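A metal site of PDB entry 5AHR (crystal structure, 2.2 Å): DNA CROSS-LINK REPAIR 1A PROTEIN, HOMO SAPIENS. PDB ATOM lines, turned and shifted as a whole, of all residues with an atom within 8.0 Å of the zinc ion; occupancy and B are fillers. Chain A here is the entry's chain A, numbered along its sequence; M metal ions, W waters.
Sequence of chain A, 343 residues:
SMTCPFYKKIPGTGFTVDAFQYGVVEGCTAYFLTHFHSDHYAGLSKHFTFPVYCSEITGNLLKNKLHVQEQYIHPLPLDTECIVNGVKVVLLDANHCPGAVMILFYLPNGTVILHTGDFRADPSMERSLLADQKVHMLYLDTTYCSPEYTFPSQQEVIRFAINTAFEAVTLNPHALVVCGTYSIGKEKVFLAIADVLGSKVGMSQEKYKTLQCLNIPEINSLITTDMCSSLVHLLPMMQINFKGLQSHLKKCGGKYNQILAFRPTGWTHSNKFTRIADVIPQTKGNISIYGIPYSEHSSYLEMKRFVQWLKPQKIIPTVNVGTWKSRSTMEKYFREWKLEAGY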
ATOM      1  N   ASP A  18      28.873  -1.251 -32.326  1.00  0.00           N
ATOM      2  CA  ASP A  18      29.294  -1.379 -30.929  1.00  0.00           C
ATOM      3  C   ASP A  18      30.758  -0.947 -30.729  1.00  0.00           C
ATOM      4  O   ASP A  18      31.508  -1.563 -29.981  1.00  0.00           O
ATOM      5  CB  ASP A  18      29.069  -2.819 -30.438  1.00  0.00           C
ATOM      6  CG  ASP A  18      27.597  -3.255 -30.552  1.00  0.00           C
ATOM      7  OD1 ASP A  18      26.719  -2.359 -30.597  1.00  0.00           O
ATOM      8  OD2 ASP A  18      27.312  -4.466 -30.593  1.00  0.00           O
ATOM      9  N   THR A  34      23.998  -2.275 -31.075  1.00  0.00           N
ATOM     10  CA  THR A  34      23.054  -3.394 -31.169  1.00  0.00           C
ATOM     11  C   THR A  34      22.189  -3.550 -29.930  1.00  0.00           C
ATOM     12  O   THR A  34      21.021  -3.944 -30.032  1.00  0.00           O
ATOM     13  CB  THR A  34      23.786  -4.733 -31.411  1.00  0.00           C
ATOM     14  OG1 THR A  34      24.684  -4.997 -30.326  1.00  0.00           O
ATOM     15  CG2 THR A  34      24.581  -4.684 -32.729  1.00  0.00           C
ATOM     16  N   HIS A  35      22.747  -3.265 -28.758  1.00  0.00           N
ATOM     17  CA  HIS A  35      21.967  -3.424 -27.529  1.00  0.00           C
ATOM     18  C   HIS A  35      22.615  -2.788 -26.317  1.00  0.00           C
ATOM     19  O   HIS A  35      23.796  -2.440 -26.336  1.00  0.00           O
ATOM     20  CB  HIS A  35      21.704  -4.921 -27.252  1.00  0.00           C
ATOM     21  CG  HIS A  35      22.927  -5.728 -26.951  1.00  0.00           C
ATOM     22  ND1 HIS A  35      23.944  -5.925 -27.864  1.00  0.00           N
ATOM     23  CD2 HIS A  35      23.276  -6.449 -25.850  1.00  0.00           C
ATOM     24  CE1 HIS A  35      24.869  -6.716 -27.340  1.00  0.00           C
ATOM     25  NE2 HIS A  35      24.486  -7.037 -26.114  1.00  0.00           N
ATOM     26  N   PHE A  36      21.812  -2.648 -25.251  1.00  0.00           N
ATOM     27  CA  PHE A  36      22.258  -1.984 -24.028  1.00  0.00           C
ATOM     28  C   PHE A  36      22.930  -2.965 -23.025  1.00  0.00           C
ATOM     29  O   PHE A  36      22.380  -3.212 -21.953  1.00  0.00           O
ATOM     30  CB  PHE A  36      21.070  -1.283 -23.373  1.00  0.00           C
ATOM     31  CG  PHE A  36      21.445  -0.245 -22.349  1.00  0.00           C
ATOM     32  CD1 PHE A  36      22.010   0.960 -22.741  1.00  0.00           C
ATOM     33  CD2 PHE A  36      21.224  -0.479 -20.995  1.00  0.00           C
ATOM     34  CE1 PHE A  36      22.366   1.927 -21.784  1.00  0.00           C
ATOM     35  CE2 PHE A  36      21.571   0.486 -20.024  1.00  0.00           C
ATOM     36  CZ  PHE A  36      22.146   1.693 -20.430  1.00  0.00           C
ATOM     37  N   HIS A  37      24.091  -3.513 -23.397  1.00  0.00           N
ATOM     38  CA  HIS A  37      24.980  -4.240 -22.476  1.00  0.00           C
ATOM     39  C   HIS A  37      26.311  -3.499 -22.416  1.00  0.00           C
ATOM     40  O   HIS A  37      26.814  -3.025 -23.446  1.00  0.00           O
ATOM     41  CB  HIS A  37      25.201  -5.704 -22.917  1.00  0.00           C
ATOM     42  CG  HIS A  37      24.095  -6.638 -22.524  1.00  0.00           C
ATOM     43  ND1 HIS A  37      23.926  -7.877 -23.108  1.00  0.00           N
ATOM     44  CD2 HIS A  37      23.104  -6.514 -21.605  1.00  0.00           C
ATOM     45  CE1 HIS A  37      22.880  -8.490 -22.562  1.00  0.00           C
ATOM     46  NE2 HIS A  37      22.359  -7.683 -21.648  1.00  0.00           N
ATOM     47  N   SER A  38      26.873  -3.375 -21.218  1.00  0.00           N
ATOM     48  CA  SER A  38      27.994  -2.452 -20.993  1.00  0.00           C
ATOM     49  C   SER A  38      29.228  -2.809 -21.823  1.00  0.00           C
ATOM     50  O   SER A  38      29.971  -1.929 -22.221  1.00  0.00           O
ATOM     51  CB  SER A  38      28.355  -2.402 -19.498  1.00  0.00           C
ATOM     52  OG  SER A  38      28.739  -3.677 -19.039  1.00  0.00           O
ATOM     53  N   ASP A  39      29.410  -4.093 -22.108  1.00  0.00           N
ATOM     54  CA  ASP A  39      30.471  -4.507 -23.042  1.00  0.00           C
ATOM     55  C   ASP A  39      30.346  -3.834 -24.407  1.00  0.00           C
ATOM     56  O   ASP A  39      31.315  -3.674 -25.127  1.00  0.00           O
ATOM     57  CB  ASP A  39      30.451  -6.028 -23.275  1.00  0.00           C
ATOM     58  CG  ASP A  39      30.974  -6.818 -22.092  1.00  0.00           C
ATOM     59  OD1 ASP A  39      31.554  -6.217 -21.156  1.00  0.00           O
ATOM     60  OD2 ASP A  39      30.816  -8.058 -22.124  1.00  0.00           O
ATOM     61  N   HIS A  40      29.118  -3.468 -24.782  1.00  0.00           N
ATOM     62  CA  HIS A  40      28.890  -2.953 -26.139  1.00  0.00           C
ATOM     63  C   HIS A  40      28.698  -1.448 -26.184  1.00  0.00           C
ATOM     64  O   HIS A  40      29.152  -0.799 -27.108  1.00  0.00           O
ATOM     65  CB  HIS A  40      27.702  -3.710 -26.765  1.00  0.00           C
ATOM     66  CG  HIS A  40      27.961  -5.174 -26.883  1.00  0.00           C
ATOM     67  ND1 HIS A  40      28.420  -5.758 -28.049  1.00  0.00           N
ATOM     68  CD2 HIS A  40      27.925  -6.168 -25.953  1.00  0.00           C
ATOM     69  CE1 HIS A  40      28.612  -7.045 -27.845  1.00  0.00           C
ATOM     70  NE2 HIS A  40      28.320  -7.322 -26.587  1.00  0.00           N
ATOM     71  N   HIS A  96      17.818 -11.641 -27.622  1.00  0.00           N
ATOM     72  CA  HIS A  96      18.941 -11.560 -26.684  1.00  0.00           C
ATOM     73  C   HIS A  96      18.515 -10.909 -25.370  1.00  0.00           C
ATOM     74  O   HIS A  96      18.535 -11.543 -24.323  1.00  0.00           O
ATOM     75  CB  HIS A  96      20.097 -10.781 -27.331  1.00  0.00           C
ATOM     76  CG  HIS A  96      21.323 -10.661 -26.467  1.00  0.00           C
ATOM     77  ND1 HIS A  96      21.976 -11.768 -25.938  1.00  0.00           N
ATOM     78  CD2 HIS A  96      22.031  -9.581 -26.067  1.00  0.00           C
ATOM     79  CE1 HIS A  96      23.026 -11.368 -25.247  1.00  0.00           C
ATOM     80  NE2 HIS A  96      23.088 -10.040 -25.304  1.00  0.00           N
ATOM     81  N   CYS A  97      18.166  -9.622 -25.436  1.00  0.00           N
ATOM     82  CA  CYS A  97      17.635  -8.863 -24.293  1.00  0.00           C
ATOM     83  C   CYS A  97      16.678  -7.803 -24.861  1.00  0.00           C
ATOM     84  O   CYS A  97      16.602  -7.654 -26.098  1.00  0.00           O
ATOM     85  CB  CYS A  97      18.782  -8.223 -23.464  1.00  0.00           C
ATOM     86  SG  CYS A  97      19.740  -6.923 -24.300  1.00  0.00           S
ATOM     87  N   ALA A 100      17.550  -5.453 -28.087  1.00  0.00           N
ATOM     88  CA  ALA A 100      18.705  -6.002 -28.803  1.00  0.00           C
ATOM     89  C   ALA A 100      18.359  -6.363 -30.242  1.00  0.00           C
ATOM     90  O   ALA A 100      17.323  -6.987 -30.496  1.00  0.00           O
ATOM     91  CB  ALA A 100      19.253  -7.247 -28.071  1.00  0.00           C
ATOM     92  N   GLY A 117      25.174  -8.959 -33.844  1.00  0.00           N
ATOM     93  CA  GLY A 117      25.381  -8.389 -32.501  1.00  0.00           C
ATOM     94  C   GLY A 117      25.494  -9.562 -31.545  1.00  0.00           C
ATOM     95  O   GLY A 117      26.062 -10.594 -31.920  1.00  0.00           O
ATOM     96  N   ASP A 118      24.957  -9.446 -30.329  1.00  0.00           N
ATOM     97  CA  ASP A 118      24.727 -10.645 -29.489  1.00  0.00           C
ATOM     98  C   ASP A 118      23.373 -11.219 -29.899  1.00  0.00           C
ATOM     99  O   ASP A 118      22.414 -10.459 -30.040  1.00  0.00           O
ATOM    100  CB  ASP A 118      24.686 -10.328 -27.993  1.00  0.00           C
ATOM    101  CG  ASP A 118      26.055 -10.086 -27.380  1.00  0.00           C
ATOM    102  OD1 ASP A 118      27.075 -10.342 -28.061  1.00  0.00           O
ATOM    103  OD2 ASP A 118      26.091  -9.644 -26.202  1.00  0.00           O
ATOM    104  N   PHE A 119      23.267 -12.551 -30.044  1.00  0.00           N
ATOM    105  CA  PHE A 119      21.957 -13.127 -30.380  1.00  0.00           C
ATOM    106  C   PHE A 119      21.804 -14.563 -29.880  1.00  0.00           C
ATOM    107  O   PHE A 119      22.783 -15.217 -29.561  1.00  0.00           O
ATOM    108  CB  PHE A 119      21.741 -12.986 -31.908  1.00  0.00           C
ATOM    109  CG  PHE A 119      22.228 -14.146 -32.767  1.00  0.00           C
ATOM    110  CD1 PHE A 119      23.521 -14.648 -32.611  1.00  0.00           C
ATOM    111  CD2 PHE A 119      21.388 -14.761 -33.682  1.00  0.00           C
ATOM    112  CE1 PHE A 119      23.978 -15.716 -33.400  1.00  0.00           C
ATOM    113  CE2 PHE A 119      21.846 -15.803 -34.503  1.00  0.00           C
ATOM    114  CZ  PHE A 119      23.143 -16.286 -34.336  1.00  0.00           C
ATOM    115  N   ASP A 141      27.994 -13.856 -33.669  1.00  0.00           N
ATOM    116  CA  ASP A 141      28.192 -14.040 -32.228  1.00  0.00           C
ATOM    117  C   ASP A 141      28.559 -15.518 -31.938  1.00  0.00           C
ATOM    118  O   ASP A 141      27.702 -16.398 -31.931  1.00  0.00           O
ATOM    119  CB  ASP A 141      26.928 -13.602 -31.484  1.00  0.00           C
ATOM    120  CG  ASP A 141      26.888 -14.072 -30.014  1.00  0.00           C
ATOM    121  OD1 ASP A 141      27.936 -14.522 -29.489  1.00  0.00           O
ATOM    122  OD2 ASP A 141      25.801 -13.964 -29.391  1.00  0.00           O
ATOM    123  N   THR A 143      29.910 -16.825 -29.146  1.00  0.00           N
ATOM    124  CA  THR A 143      30.078 -17.044 -27.709  1.00  0.00           C
ATOM    125  C   THR A 143      30.181 -18.523 -27.328  1.00  0.00           C
ATOM    126  O   THR A 143      31.135 -18.938 -26.668  1.00  0.00           O
ATOM    127  CB  THR A 143      28.925 -16.377 -26.925  1.00  0.00           C
ATOM    128  OG1 THR A 143      28.954 -14.967 -27.140  1.00  0.00           O
ATOM    129  CG2 THR A 143      29.044 -16.665 -25.435  1.00  0.00           C
ATOM    130  N   GLU A 296      21.276 -16.085 -22.839  1.00  0.00           N
ATOM    131  CA  GLU A 296      20.868 -15.102 -23.847  1.00  0.00           C
ATOM    132  C   GLU A 296      21.654 -15.266 -25.146  1.00  0.00           C
ATOM    133  O   GLU A 296      21.527 -14.442 -26.062  1.00  0.00           O
ATOM    134  CB  GLU A 296      21.039 -13.689 -23.269  1.00  0.00           C
ATOM    135  CG  GLU A 296      20.140 -13.480 -22.046  1.00  0.00           C
ATOM    136  CD  GLU A 296      20.335 -12.127 -21.343  1.00  0.00           C
ATOM    137  OE1 GLU A 296      21.380 -11.464 -21.545  1.00  0.00           O
ATOM    138  OE2 GLU A 296      19.428 -11.741 -20.577  1.00  0.00           O
ATOM    139  N   HIS A 297      22.464 -16.335 -25.213  1.00  0.00           N
ATOM    140  CA  HIS A 297      23.239 -16.644 -26.411  1.00  0.00           C
ATOM    141  C   HIS A 297      22.896 -18.021 -26.994  1.00  0.00           C
ATOM    142  O   HIS A 297      22.516 -18.917 -26.243  1.00  0.00           O
ATOM    143  CB  HIS A 297      24.742 -16.620 -26.101  1.00  0.00           C
ATOM    144  CG  HIS A 297      25.274 -15.280 -25.728  1.00  0.00           C
ATOM    145  ND1 HIS A 297      25.742 -14.370 -26.664  1.00  0.00           N
ATOM    146  CD2 HIS A 297      25.448 -14.685 -24.519  1.00  0.00           C
ATOM    147  CE1 HIS A 297      26.178 -13.288 -26.045  1.00  0.00           C
ATOM    148  NE2 HIS A 297      26.007 -13.453 -24.743  1.00  0.00           N
HETATM  149 ZN    ZN M   1      24.876  -8.824 -24.707  1.00  0.00          ZN
HETATM  150  O   HOH W   1      25.606 -10.610 -23.287  1.00  0.00           O
HETATM  151  O   HOH W   2      26.861  -8.108 -24.153  1.00  0.00           O
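The zinc ion is bound by a ring nitrogen (ND1) of His 37 (2.1 Å), the side-chain carboxylate of Asp 118 (2.1 Å), water W2 (2.2 Å), a ring nitrogen (NE2) of His 96 (2.2 Å), a ring nitrogen (NE2) of His 35 (2.3 Å) and water W1 (2.4 Å). The zinc ion has six donor atoms within binding distance.
The side-chain carboxylate of Asp 118 lies close to a ring nitrogen (NE2) of His 40. The backbone carbonyl oxygen (O) of Glu 296 is in hydrogen-bond range of a ring nitrogen (ND1) of His 96 (2.7 Å). The side-chain hydroxyl of Thr 34 sits at hydrogen-bond distance from a ring nitrogen (ND1) of His 35.
Within 4 Å of the zinc ion: His 35, His 37, His 96 and Asp 118. Along chain A the residues within 4 Å of the zinc ion span positions 35 to 118. The nearest printed residue that does not touch the zinc ion is His 40 (4.2 Å).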
